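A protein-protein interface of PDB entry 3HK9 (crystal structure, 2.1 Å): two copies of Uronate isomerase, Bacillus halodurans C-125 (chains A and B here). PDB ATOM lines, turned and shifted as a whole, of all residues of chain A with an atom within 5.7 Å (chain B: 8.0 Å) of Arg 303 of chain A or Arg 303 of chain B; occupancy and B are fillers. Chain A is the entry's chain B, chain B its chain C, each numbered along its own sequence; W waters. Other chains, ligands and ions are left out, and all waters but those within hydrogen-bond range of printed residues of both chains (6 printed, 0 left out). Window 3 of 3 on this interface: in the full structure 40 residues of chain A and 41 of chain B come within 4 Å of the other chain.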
ATOM      1  N   VAL A 276       3.184  30.736 -17.027  1.00  0.00           N
ATOM      2  CA  VAL A 276       2.623  29.520 -16.431  1.00  0.00           C
ATOM      3  C   VAL A 276       3.008  29.359 -14.965  1.00  0.00           C
ATOM      4  O   VAL A 276       4.016  29.898 -14.515  1.00  0.00           O
ATOM      5  CB  VAL A 276       3.119  28.252 -17.200  1.00  0.00           C
ATOM      6  CG1 VAL A 276       4.648  28.214 -17.207  1.00  0.00           C
ATOM      7  CG2 VAL A 276       2.580  26.971 -16.543  1.00  0.00           C
ATOM      8  N   LEU A 301      -1.321  23.407 -17.603  1.00  0.00           N
ATOM      9  CA  LEU A 301      -0.180  24.057 -18.252  1.00  0.00           C
ATOM     10  C   LEU A 301       1.217  23.764 -17.705  1.00  0.00           C
ATOM     11  O   LEU A 301       2.202  23.804 -18.455  1.00  0.00           O
ATOM     12  CB  LEU A 301      -0.423  25.573 -18.274  1.00  0.00           C
ATOM     13  CG  LEU A 301       0.407  26.442 -19.218  1.00  0.00           C
ATOM     14  CD1 LEU A 301       0.225  25.960 -20.653  1.00  0.00           C
ATOM     15  CD2 LEU A 301      -0.030  27.890 -19.089  1.00  0.00           C
ATOM     16  N   SER A 302       1.301  23.471 -16.413  1.00  0.00           N
ATOM     17  CA  SER A 302       2.578  23.192 -15.757  1.00  0.00           C
ATOM     18  C   SER A 302       3.069  21.756 -15.946  1.00  0.00           C
ATOM     19  O   SER A 302       2.316  20.806 -15.729  1.00  0.00           O
ATOM     20  CB  SER A 302       2.456  23.476 -14.256  1.00  0.00           C
ATOM     21  OG  SER A 302       3.643  23.130 -13.556  1.00  0.00           O
ATOM     22  N   ARG A 303       4.334  21.600 -16.332  1.00  0.00           N
ATOM     23  CA  ARG A 303       4.920  20.265 -16.503  1.00  0.00           C
ATOM     24  C   ARG A 303       4.788  19.519 -15.183  1.00  0.00           C
ATOM     25  O   ARG A 303       4.536  18.315 -15.152  1.00  0.00           O
ATOM     26  CB  ARG A 303       6.410  20.361 -16.853  1.00  0.00           C
ATOM     27  CG  ARG A 303       7.082  19.007 -17.100  1.00  0.00           C
ATOM     28  CD  ARG A 303       8.607  19.100 -17.078  1.00  0.00           C
ATOM     29  NE  ARG A 303       9.239  17.828 -17.440  1.00  0.00           N
ATOM     30  CZ  ARG A 303      10.516  17.528 -17.219  1.00  0.00           C
ATOM     31  NH1 ARG A 303      11.318  18.401 -16.624  1.00  0.00           N
ATOM     32  NH2 ARG A 303      10.998  16.354 -17.610  1.00  0.00           N
ATOM     33  N   GLU A 304       4.962  20.254 -14.089  1.00  0.00           N
ATOM     34  CA  GLU A 304       4.893  19.694 -12.745  1.00  0.00           C
ATOM     35  C   GLU A 304       3.514  19.225 -12.267  1.00  0.00           C
ATOM     36  O   GLU A 304       3.410  18.604 -11.208  1.00  0.00           O
ATOM     37  CB  GLU A 304       5.482  20.694 -11.745  1.00  0.00           C
ATOM     38  CG  GLU A 304       7.003  20.859 -11.855  1.00  0.00           C
ATOM     39  CD  GLU A 304       7.448  21.388 -13.204  1.00  0.00           C
ATOM     40  OE1 GLU A 304       6.937  22.452 -13.619  1.00  0.00           O
ATOM     41  OE2 GLU A 304       8.315  20.745 -13.848  1.00  0.00           O
ATOM     42  N   ASN A 305       2.470  19.496 -13.048  1.00  0.00           N
ATOM     43  CA  ASN A 305       1.101  19.087 -12.703  1.00  0.00           C
ATOM     44  C   ASN A 305       0.695  17.797 -13.442  1.00  0.00           C
ATOM     45  O   ASN A 305      -0.229  17.084 -13.026  1.00  0.00           O
ATOM     46  CB  ASN A 305       0.091  20.182 -13.110  1.00  0.00           C
ATOM     47  CG  ASN A 305      -0.162  21.219 -12.020  1.00  0.00           C
ATOM     48  OD1 ASN A 305      -0.244  22.418 -12.309  1.00  0.00           O
ATOM     49  ND2 ASN A 305      -0.321  20.766 -10.775  1.00  0.00           N
ATOM     50  N   GLN A 306       1.396  17.490 -14.528  1.00  0.00           N
ATOM     51  CA  GLN A 306       1.037  16.341 -15.361  1.00  0.00           C
ATOM     52  C   GLN A 306       0.918  14.954 -14.726  1.00  0.00           C
ATOM     53  O   GLN A 306      -0.058  14.243 -14.988  1.00  0.00           O
ATOM     54  CB  GLN A 306       1.967  16.271 -16.571  1.00  0.00           C
ATOM     55  CG  GLN A 306       1.999  17.545 -17.420  1.00  0.00           C
ATOM     56  CD  GLN A 306       0.613  18.094 -17.783  1.00  0.00           C
ATOM     57  OE1 GLN A 306      -0.332  17.346 -18.052  1.00  0.00           O
ATOM     58  NE2 GLN A 306       0.506  19.415 -17.817  1.00  0.00           N
ATOM     59  N   HIS A 307       1.889  14.549 -13.911  1.00  0.00           N
ATOM     60  CA  HIS A 307       1.805  13.219 -13.308  1.00  0.00           C
ATOM     61  C   HIS A 307       0.635  13.078 -12.338  1.00  0.00           C
ATOM     62  O   HIS A 307      -0.137  12.123 -12.444  1.00  0.00           O
ATOM     63  CB  HIS A 307       3.114  12.830 -12.599  1.00  0.00           C
ATOM     64  CG  HIS A 307       3.049  11.490 -11.922  1.00  0.00           C
ATOM     65  ND1 HIS A 307       2.606  11.331 -10.627  1.00  0.00           N
ATOM     66  CD2 HIS A 307       3.281  10.241 -12.393  1.00  0.00           C
ATOM     67  CE1 HIS A 307       2.562  10.043 -10.330  1.00  0.00           C
ATOM     68  NE2 HIS A 307       2.965   9.361 -11.387  1.00  0.00           N
ATOM     69  N   MET A 328       3.302  22.714 -23.041  1.00  0.00           N
ATOM     70  CA  MET A 328       3.425  21.264 -22.897  1.00  0.00           C
ATOM     71  C   MET A 328       3.518  20.663 -24.303  1.00  0.00           C
ATOM     72  O   MET A 328       3.954  19.527 -24.481  1.00  0.00           O
ATOM     73  CB  MET A 328       2.190  20.664 -22.205  1.00  0.00           C
ATOM     74  CG  MET A 328       1.944  21.116 -20.781  1.00  0.00           C
ATOM     75  SD  MET A 328       3.198  20.532 -19.616  1.00  0.00           S
ATOM     76  CE  MET A 328       4.302  21.935 -19.593  1.00  0.00           C
ATOM     77  N   GLU A 332       9.472  16.671 -26.231  1.00  0.00           N
ATOM     78  CA  GLU A 332       9.984  16.125 -24.972  1.00  0.00           C
ATOM     79  C   GLU A 332       8.870  15.932 -23.945  1.00  0.00           C
ATOM     80  O   GLU A 332       8.817  14.912 -23.246  1.00  0.00           O
ATOM     81  CB  GLU A 332      11.065  17.058 -24.397  1.00  0.00           C
ATOM     82  CG  GLU A 332      11.699  16.606 -23.082  1.00  0.00           C
ATOM     83  CD  GLU A 332      12.545  15.345 -23.212  1.00  0.00           C
ATOM     84  OE1 GLU A 332      12.841  14.934 -24.351  1.00  0.00           O
ATOM     85  OE2 GLU A 332      12.925  14.770 -22.168  1.00  0.00           O
ATOM     86  N   ILE A 333       7.981  16.917 -23.855  1.00  0.00           N
ATOM     87  CA  ILE A 333       6.881  16.850 -22.903  1.00  0.00           C
ATOM     88  C   ILE A 333       5.737  15.990 -23.427  1.00  0.00           C
ATOM     89  O   ILE A 333       5.131  15.229 -22.670  1.00  0.00           O
ATOM     90  CB  ILE A 333       6.357  18.269 -22.559  1.00  0.00           C
ATOM     91  CG1 ILE A 333       7.514  19.138 -22.054  1.00  0.00           C
ATOM     92  CG2 ILE A 333       5.252  18.184 -21.510  1.00  0.00           C
ATOM     93  CD1 ILE A 333       8.232  18.558 -20.864  1.00  0.00           C
ATOM     94  N   GLU A 336       6.751  12.295 -22.750  1.00  0.00           N
ATOM     95  CA  GLU A 336       6.651  11.854 -21.363  1.00  0.00           C
ATOM     96  C   GLU A 336       5.206  11.871 -20.861  1.00  0.00           C
ATOM     97  O   GLU A 336       4.798  11.001 -20.088  1.00  0.00           O
ATOM     98  CB  GLU A 336       7.543  12.710 -20.449  1.00  0.00           C
ATOM     99  CG  GLU A 336       6.968  14.060 -19.992  1.00  0.00           C
ATOM    100  CD  GLU A 336       7.968  14.840 -19.135  1.00  0.00           C
ATOM    101  OE1 GLU A 336       7.583  15.848 -18.505  1.00  0.00           O
ATOM    102  OE2 GLU A 336       9.149  14.438 -19.097  1.00  0.00           O
ATOM    103  N   VAL B 276      19.020  21.506  -1.978  1.00  0.00           N
ATOM    104  CA  VAL B 276      18.257  22.188  -3.025  1.00  0.00           C
ATOM    105  C   VAL B 276      16.772  22.343  -2.705  1.00  0.00           C
ATOM    106  O   VAL B 276      16.209  21.558  -1.946  1.00  0.00           O
ATOM    107  CB  VAL B 276      18.359  21.428  -4.377  1.00  0.00           C
ATOM    108  CG1 VAL B 276      17.786  20.011  -4.234  1.00  0.00           C
ATOM    109  CG2 VAL B 276      17.599  22.179  -5.468  1.00  0.00           C
ATOM    110  N   GLY B 277      16.145  23.343  -3.319  1.00  0.00           N
ATOM    111  CA  GLY B 277      14.727  23.583  -3.112  1.00  0.00           C
ATOM    112  C   GLY B 277      14.125  24.317  -4.298  1.00  0.00           C
ATOM    113  O   GLY B 277      14.803  25.118  -4.943  1.00  0.00           O
ATOM    114  N   LYS B 278      12.858  24.044  -4.595  1.00  0.00           N
ATOM    115  CA  LYS B 278      12.174  24.705  -5.704  1.00  0.00           C
ATOM    116  C   LYS B 278      11.877  26.148  -5.312  1.00  0.00           C
ATOM    117  O   LYS B 278      11.449  26.425  -4.191  1.00  0.00           O
ATOM    118  CB  LYS B 278      10.858  23.988  -6.028  1.00  0.00           C
ATOM    119  CG  LYS B 278      10.127  24.571  -7.229  1.00  0.00           C
ATOM    120  CD  LYS B 278       8.767  23.923  -7.447  1.00  0.00           C
ATOM    121  CE  LYS B 278       8.123  24.446  -8.731  1.00  0.00           C
ATOM    122  NZ  LYS B 278       6.811  23.781  -9.014  1.00  0.00           N
ATOM    123  N   MET B 300      18.951  27.718 -12.495  1.00  0.00           N
ATOM    124  CA  MET B 300      18.304  27.265 -11.267  1.00  0.00           C
ATOM    125  C   MET B 300      18.687  25.838 -10.870  1.00  0.00           C
ATOM    126  O   MET B 300      19.010  24.998 -11.718  1.00  0.00           O
ATOM    127  CB  MET B 300      16.787  27.425 -11.405  1.00  0.00           C
ATOM    128  CG  MET B 300      16.393  28.880 -11.673  1.00  0.00           C
ATOM    129  SD  MET B 300      14.632  29.184 -11.780  1.00  0.00           S
ATOM    130  CE  MET B 300      14.192  29.124 -10.021  1.00  0.00           C
ATOM    131  N   LEU B 301      18.636  25.577  -9.569  1.00  0.00           N
ATOM    132  CA  LEU B 301      19.032  24.291  -9.020  1.00  0.00           C
ATOM    133  C   LEU B 301      17.996  23.166  -8.966  1.00  0.00           C
ATOM    134  O   LEU B 301      18.359  21.993  -9.013  1.00  0.00           O
ATOM    135  CB  LEU B 301      19.593  24.514  -7.616  1.00  0.00           C
ATOM    136  CG  LEU B 301      20.399  23.362  -7.007  1.00  0.00           C
ATOM    137  CD1 LEU B 301      21.579  23.018  -7.916  1.00  0.00           C
ATOM    138  CD2 LEU B 301      20.890  23.774  -5.625  1.00  0.00           C
ATOM    139  N   SER B 302      16.719  23.508  -8.851  1.00  0.00           N
ATOM    140  CA  SER B 302      15.686  22.485  -8.752  1.00  0.00           C
ATOM    141  C   SER B 302      15.227  21.947 -10.096  1.00  0.00           C
ATOM    142  O   SER B 302      15.021  22.705 -11.033  1.00  0.00           O
ATOM    143  CB  SER B 302      14.485  23.046  -7.983  1.00  0.00           C
ATOM    144  OG  SER B 302      13.383  22.156  -8.009  1.00  0.00           O
ATOM    145  N   ARG B 303      15.054  20.633 -10.188  1.00  0.00           N
ATOM    146  CA  ARG B 303      14.598  20.024 -11.430  1.00  0.00           C
ATOM    147  C   ARG B 303      13.246  20.605 -11.827  1.00  0.00           C
ATOM    148  O   ARG B 303      12.968  20.853 -13.005  1.00  0.00           O
ATOM    149  CB  ARG B 303      14.442  18.508 -11.263  1.00  0.00           C
ATOM    150  CG  ARG B 303      13.975  17.805 -12.539  1.00  0.00           C
ATOM    151  CD  ARG B 303      13.568  16.361 -12.291  1.00  0.00           C
ATOM    152  NE  ARG B 303      13.262  15.673 -13.542  1.00  0.00           N
ATOM    153  CZ  ARG B 303      12.589  14.531 -13.627  1.00  0.00           C
ATOM    154  NH1 ARG B 303      12.139  13.939 -12.529  1.00  0.00           N
ATOM    155  NH2 ARG B 303      12.375  13.971 -14.814  1.00  0.00           N
ATOM    156  N   GLU B 304      12.419  20.826 -10.811  1.00  0.00           N
ATOM    157  CA  GLU B 304      11.063  21.328 -10.977  1.00  0.00           C
ATOM    158  C   GLU B 304      10.906  22.801 -11.397  1.00  0.00           C
ATOM    159  O   GLU B 304       9.789  23.271 -11.599  1.00  0.00           O
ATOM    160  CB  GLU B 304      10.285  21.053  -9.686  1.00  0.00           C
ATOM    161  CG  GLU B 304      10.050  19.556  -9.374  1.00  0.00           C
ATOM    162  CD  GLU B 304      11.335  18.745  -9.164  1.00  0.00           C
ATOM    163  OE1 GLU B 304      12.174  19.123  -8.318  1.00  0.00           O
ATOM    164  OE2 GLU B 304      11.505  17.712  -9.842  1.00  0.00           O
ATOM    165  N   ASN B 305      12.019  23.518 -11.538  1.00  0.00           N
ATOM    166  CA  ASN B 305      11.997  24.929 -11.953  1.00  0.00           C
ATOM    167  C   ASN B 305      12.413  25.046 -13.423  1.00  0.00           C
ATOM    168  O   ASN B 305      12.187  26.075 -14.060  1.00  0.00           O
ATOM    169  CB  ASN B 305      13.016  25.750 -11.144  1.00  0.00           C
ATOM    170  CG  ASN B 305      12.448  26.345  -9.863  1.00  0.00           C
ATOM    171  OD1 ASN B 305      13.166  26.459  -8.871  1.00  0.00           O
ATOM    172  ND2 ASN B 305      11.184  26.757  -9.885  1.00  0.00           N
ATOM    173  N   GLN B 306      13.023  23.992 -13.957  1.00  0.00           N
ATOM    174  CA  GLN B 306      13.555  24.038 -15.318  1.00  0.00           C
ATOM    175  C   GLN B 306      12.619  24.388 -16.458  1.00  0.00           C
ATOM    176  O   GLN B 306      12.986  25.178 -17.336  1.00  0.00           O
ATOM    177  CB  GLN B 306      14.277  22.726 -15.660  1.00  0.00           C
ATOM    178  CG  GLN B 306      15.487  22.406 -14.772  1.00  0.00           C
ATOM    179  CD  GLN B 306      16.374  23.616 -14.472  1.00  0.00           C
ATOM    180  OE1 GLN B 306      16.636  24.453 -15.343  1.00  0.00           O
ATOM    181  NE2 GLN B 306      16.860  23.695 -13.233  1.00  0.00           N
ATOM    182  N   HIS B 307      11.423  23.806 -16.465  1.00  0.00           N
ATOM    183  CA  HIS B 307      10.485  24.077 -17.545  1.00  0.00           C
ATOM    184  C   HIS B 307       9.952  25.499 -17.509  1.00  0.00           C
ATOM    185  O   HIS B 307       9.995  26.201 -18.518  1.00  0.00           O
ATOM    186  CB  HIS B 307       9.318  23.084 -17.517  1.00  0.00           C
ATOM    187  CG  HIS B 307       8.255  23.383 -18.529  1.00  0.00           C
ATOM    188  ND1 HIS B 307       7.170  24.183 -18.248  1.00  0.00           N
ATOM    189  CD2 HIS B 307       8.142  23.037 -19.834  1.00  0.00           C
ATOM    190  CE1 HIS B 307       6.433  24.319 -19.336  1.00  0.00           C
ATOM    191  NE2 HIS B 307       7.001  23.634 -20.314  1.00  0.00           N
ATOM    192  N   GLU B 308       9.451  25.928 -16.356  1.00  0.00           N
ATOM    193  CA  GLU B 308       8.919  27.283 -16.246  1.00  0.00           C
ATOM    194  C   GLU B 308       9.997  28.348 -16.484  1.00  0.00           C
ATOM    195  O   GLU B 308       9.681  29.460 -16.904  1.00  0.00           O
ATOM    196  CB  GLU B 308       8.238  27.484 -14.886  1.00  0.00           C
ATOM    197  CG  GLU B 308       9.079  27.102 -13.670  1.00  0.00           C
ATOM    198  CD  GLU B 308       8.231  26.976 -12.411  1.00  0.00           C
ATOM    199  OE1 GLU B 308       6.991  26.837 -12.548  1.00  0.00           O
ATOM    200  OE2 GLU B 308       8.797  26.997 -11.292  1.00  0.00           O
ATOM    201  N   VAL B 311      10.012  28.851 -20.077  1.00  0.00           N
ATOM    202  CA  VAL B 311       8.850  29.633 -20.477  1.00  0.00           C
ATOM    203  C   VAL B 311       9.052  31.110 -20.155  1.00  0.00           C
ATOM    204  O   VAL B 311       8.649  31.978 -20.930  1.00  0.00           O
ATOM    205  CB  VAL B 311       7.568  29.130 -19.772  1.00  0.00           C
ATOM    206  CG1 VAL B 311       6.359  29.931 -20.256  1.00  0.00           C
ATOM    207  CG2 VAL B 311       7.366  27.650 -20.070  1.00  0.00           C
ATOM    208  N   TRP B 325      23.084  23.429 -13.930  1.00  0.00           N
ATOM    209  CA  TRP B 325      23.803  23.633 -12.686  1.00  0.00           C
ATOM    210  C   TRP B 325      23.799  22.582 -11.581  1.00  0.00           C
ATOM    211  O   TRP B 325      22.746  22.102 -11.159  1.00  0.00           O
ATOM    212  CB  TRP B 325      23.335  24.978 -12.097  1.00  0.00           C
ATOM    213  CG  TRP B 325      24.064  25.460 -10.860  1.00  0.00           C
ATOM    214  CD1 TRP B 325      25.402  25.370 -10.605  1.00  0.00           C
ATOM    215  CD2 TRP B 325      23.496  26.195  -9.762  1.00  0.00           C
ATOM    216  NE1 TRP B 325      25.702  26.007  -9.422  1.00  0.00           N
ATOM    217  CE2 TRP B 325      24.552  26.521  -8.885  1.00  0.00           C
ATOM    218  CE3 TRP B 325      22.199  26.612  -9.440  1.00  0.00           C
ATOM    219  CZ2 TRP B 325      24.352  27.246  -7.704  1.00  0.00           C
ATOM    220  CZ3 TRP B 325      21.999  27.333  -8.266  1.00  0.00           C
ATOM    221  CH2 TRP B 325      23.072  27.641  -7.414  1.00  0.00           C
ATOM    222  N   PHE B 327      23.308  19.946  -9.266  1.00  0.00           N
ATOM    223  CA  PHE B 327      22.481  18.748  -9.214  1.00  0.00           C
ATOM    224  C   PHE B 327      21.744  18.497 -10.524  1.00  0.00           C
ATOM    225  O   PHE B 327      21.134  17.444 -10.710  1.00  0.00           O
ATOM    226  CB  PHE B 327      21.508  18.849  -8.035  1.00  0.00           C
ATOM    227  CG  PHE B 327      22.201  19.044  -6.718  1.00  0.00           C
ATOM    228  CD1 PHE B 327      23.209  18.164  -6.315  1.00  0.00           C
ATOM    229  CD2 PHE B 327      21.903  20.134  -5.909  1.00  0.00           C
ATOM    230  CE1 PHE B 327      23.915  18.374  -5.125  1.00  0.00           C
ATOM    231  CE2 PHE B 327      22.606  20.351  -4.717  1.00  0.00           C
ATOM    232  CZ  PHE B 327      23.614  19.467  -4.329  1.00  0.00           C
ATOM    233  N   MET B 328      21.812  19.467 -11.433  1.00  0.00           N
ATOM    234  CA  MET B 328      21.189  19.341 -12.745  1.00  0.00           C
ATOM    235  C   MET B 328      22.232  18.785 -13.723  1.00  0.00           C
ATOM    236  O   MET B 328      21.890  18.287 -14.796  1.00  0.00           O
ATOM    237  CB  MET B 328      20.732  20.715 -13.272  1.00  0.00           C
ATOM    238  CG  MET B 328      19.672  21.420 -12.451  1.00  0.00           C
ATOM    239  SD  MET B 328      18.072  20.604 -12.525  1.00  0.00           S
ATOM    240  CE  MET B 328      18.171  19.582 -11.056  1.00  0.00           C
ATOM    241  N   GLU B 332      20.789  12.429 -17.403  1.00  0.00           N
ATOM    242  CA  GLU B 332      19.329  12.371 -17.528  1.00  0.00           C
ATOM    243  C   GLU B 332      18.698  13.773 -17.495  1.00  0.00           C
ATOM    244  O   GLU B 332      17.775  14.067 -18.262  1.00  0.00           O
ATOM    245  CB  GLU B 332      18.743  11.501 -16.411  1.00  0.00           C
ATOM    246  CG  GLU B 332      17.224  11.368 -16.404  1.00  0.00           C
ATOM    247  CD  GLU B 332      16.666  10.630 -17.616  1.00  0.00           C
ATOM    248  OE1 GLU B 332      17.444  10.016 -18.373  1.00  0.00           O
ATOM    249  OE2 GLU B 332      15.435  10.659 -17.805  1.00  0.00           O
ATOM    250  N   ILE B 333      19.203  14.635 -16.616  1.00  0.00           N
ATOM    251  CA  ILE B 333      18.685  15.999 -16.496  1.00  0.00           C
ATOM    252  C   ILE B 333      19.168  16.904 -17.638  1.00  0.00           C
ATOM    253  O   ILE B 333      18.375  17.629 -18.241  1.00  0.00           O
ATOM    254  CB  ILE B 333      19.082  16.614 -15.132  1.00  0.00           C
ATOM    255  CG1 ILE B 333      18.570  15.716 -13.999  1.00  0.00           C
ATOM    256  CG2 ILE B 333      18.506  18.024 -14.987  1.00  0.00           C
ATOM    257  CD1 ILE B 333      17.075  15.392 -14.089  1.00  0.00           C
ATOM    258  N   GLU B 336      17.040  16.237 -20.800  1.00  0.00           N
ATOM    259  CA  GLU B 336      15.680  16.767 -20.792  1.00  0.00           C
ATOM    260  C   GLU B 336      15.666  18.294 -20.791  1.00  0.00           C
ATOM    261  O   GLU B 336      14.807  18.910 -21.429  1.00  0.00           O
ATOM    262  CB  GLU B 336      14.880  16.210 -19.596  1.00  0.00           C
ATOM    263  CG  GLU B 336      15.064  16.937 -18.272  1.00  0.00           C
ATOM    264  CD  GLU B 336      14.269  16.299 -17.130  1.00  0.00           C
ATOM    265  OE1 GLU B 336      14.154  16.922 -16.056  1.00  0.00           O
ATOM    266  OE2 GLU B 336      13.762  15.172 -17.300  1.00  0.00           O
ATOM    267  N   MET B 337      16.622  18.898 -20.090  1.00  0.00           N
ATOM    268  CA  MET B 337      16.703  20.352 -20.021  1.00  0.00           C
ATOM    269  C   MET B 337      17.068  20.933 -21.372  1.00  0.00           C
ATOM    270  O   MET B 337      16.448  21.887 -21.838  1.00  0.00           O
ATOM    271  CB  MET B 337      17.749  20.797 -18.994  1.00  0.00           C
ATOM    272  CG  MET B 337      17.321  20.674 -17.546  1.00  0.00           C
ATOM    273  SD  MET B 337      18.620  21.257 -16.428  1.00  0.00           S
ATOM    274  CE  MET B 337      18.734  23.002 -16.951  1.00  0.00           C
ATOM    275  N   MET B 340      13.990  20.640 -23.791  1.00  0.00           N
ATOM    276  CA  MET B 340      12.916  21.603 -23.538  1.00  0.00           C
ATOM    277  C   MET B 340      13.358  22.996 -23.992  1.00  0.00           C
ATOM    278  O   MET B 340      12.608  23.707 -24.649  1.00  0.00           O
ATOM    279  CB  MET B 340      12.567  21.653 -22.054  1.00  0.00           C
ATOM    280  CG  MET B 340      11.994  20.352 -21.494  1.00  0.00           C
ATOM    281  SD  MET B 340      11.278  20.569 -19.836  1.00  0.00           S
ATOM    282  CE  MET B 340      12.755  20.686 -18.829  1.00  0.00           C
ATOM    283  N   MET B 344      11.634  25.256 -27.170  1.00  0.00           N
ATOM    284  CA  MET B 344      10.911  26.507 -26.936  1.00  0.00           C
ATOM    285  C   MET B 344      11.722  27.782 -27.200  1.00  0.00           C
ATOM    286  O   MET B 344      11.151  28.867 -27.288  1.00  0.00           O
ATOM    287  CB  MET B 344      10.360  26.552 -25.500  1.00  0.00           C
ATOM    288  CG  MET B 344       9.021  25.821 -25.294  1.00  0.00           C
ATOM    289  SD  MET B 344       8.362  25.923 -23.586  1.00  0.00           S
ATOM    290  CE  MET B 344       9.357  24.602 -22.814  1.00  0.00           C
HETATM  291  O   HOH W   1       4.793  25.877 -13.987  1.00  0.00           O
HETATM  292  O   HOH W   2      10.910  21.234 -14.994  1.00  0.00           O
HETATM  293  O   HOH W   3       9.208  24.017 -14.134  1.00  0.00           O
HETATM  294  O   HOH W   4       6.196  23.970 -15.944  1.00  0.00           O
HETATM  295  O   HOH W   5       6.193  24.290 -11.794  1.00  0.00           O
HETATM  296  O   HOH W   6      14.188  19.599 -15.607  1.00  0.00           O
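The guanidinium group of Arg 303 of chain A lies within salt-bridge range of the side-chain carboxylate of Glu 336 of chain B (3.0 Å).
NE of Arg 303 of chain B is in salt-bridge range of OE1 of Glu 336 of chain B (2.9 Å). The guanidinium group of Arg 303 of chain A is in salt-bridge range of the side-chain carboxylate of Glu 336 of chain A. NE2 of Gln 306 of chain A sits at hydrogen-bond distance from SD of Met 328 of chain A, at 3.4 Å. The backbone NH (N) of Arg 303 of chain A sits close to the side-chain sulfur (SD) of Met 328 of chain A, at 3.6 Å. The side-chain hydroxyl (OG) of Ser 302 of chain A sits close to the backbone NH (N) of Glu 304 of chain A (3.2 Å). OG of Ser 302 of chain B lies close to N of Glu 304 of chain B, at 3.2 Å.
Val 276 of chain A touches Val 311 of chain B (CG1 to CG1, 3.9 Å). Arg 303 of chain A touches Arg 303 of chain B. Arg 303 of chain A touches His 307 of chain B. CE of Met 340 of chain B touches NH1 of Arg 303 of chain A, 3.5 Å away. Glu 304 of chain B touches Glu 304 of chain A (O to CD, 3.4 Å). His 307 of chain B touches Met 328 of chain A (CE1 to CE, 3.2 Å). Glu 336 of chain B touches Glu 332 of chain A. Met 340 of chain B touches Ile 333 of chain A.
Of the printed residues of chain B, Arg 303 of chain A touches Arg 303 (3.9 Å), His 307 (3.9 Å), Glu 336 (3.0 Å) and Met 340 (3.5 Å). Arg 303 of chain B touches one residue of chain A. No residue of chain B comes within 4 Å of Ser 302 of chain A. Of the printed residues of chain A, His 307 of chain B touches Arg 303 (3.9 Å) and Met 328 (3.2 Å). Of the printed residues of chain A, Glu 304 of chain B touches Glu 304. Printed residues of chain A within 4 Å of Glu 336 of chain B: Arg 303 (3.0 Å) and Glu 332 (3.5 Å). Printed residues of chain A within 4 Å of Met 340 of chain B: Arg 303 (3.5 Å) and Ile 333 (3.8 Å). Glu 332 of chain B touches none of the printed residues of chain A. Phe 327 of chain B touches none of the printed residues of chain A.
Of the 12 printed residues of chain A, 6 touch a printed residue of chain B. Printed residues of chain A that touch a printed residue of chain B: Val 276, Arg 303, Glu 304, Met 328, Glu 332 and Ile 333. Hydrophobic or aromatic side chains of chain A within 4 Å of the printed part of chain B: Val 276, Met 328 and Ile 333. Hydrophobic or aromatic side chains of chain B within 4 Å of the printed part of chain A: His 307, Val 311 and Met 340. Among the printed residues, Asp or Glu carboxylates within 4 Å of a Lys or Arg side-chain nitrogen of the other chain: Arg 303 of chain A with Glu 336 of chain B (3.0 Å).
Arg 303 of chain A touches its own counterpart, Arg 303 of chain B. Arg 303 of chain A touches Glu 336 of chain B, but with the chains exchanged Glu 336 of chain A does not touch Arg 303 of chain B (5.4 Å). Met 328 of chain A touches His 307 of chain B, but with the chains exchanged His 307 of chain A does not touch Met 328 of chain B (16.6 Å). Glu 332 of chain A touches Glu 336 of chain B, but with the chains exchanged Glu 336 of chain A does not touch Glu 332 of chain B (7.4 Å). Positions printed for both chains: 276, 301, 302, 303, 304, 305, 306, 307, 328, 332, 333 and 336.
Water W5 lies within hydrogen-bond range of OE1 of Glu 304 of chain A (2.7 Å), OE1 of Glu 308 of chain B (2.8 Å), NZ of Lys 278 of chain B (2.9 Å) and OG of Ser 302 of chain A (3.3 Å). Water W3 lies within hydrogen-bond range of the backbone carbonyl oxygen (O) of Glu 304 of chain B (2.7 Å), the side-chain carboxylate (OE1) of Glu 304 of chain A (2.8 Å), the backbone NH (N) of Glu 308 of chain B (2.9 Å) and the backbone NH (N) of His 307 of chain B (3.2 Å). Water W2 lies within hydrogen-bond range of the side-chain carboxylate (OE2) of Glu 304 of chain A, the backbone carbonyl oxygen (O) of Arg 303 of chain B, the backbone NH (N) of His 307 of chain B and the guanidinium group (NH1) of Arg 303 of chain A.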
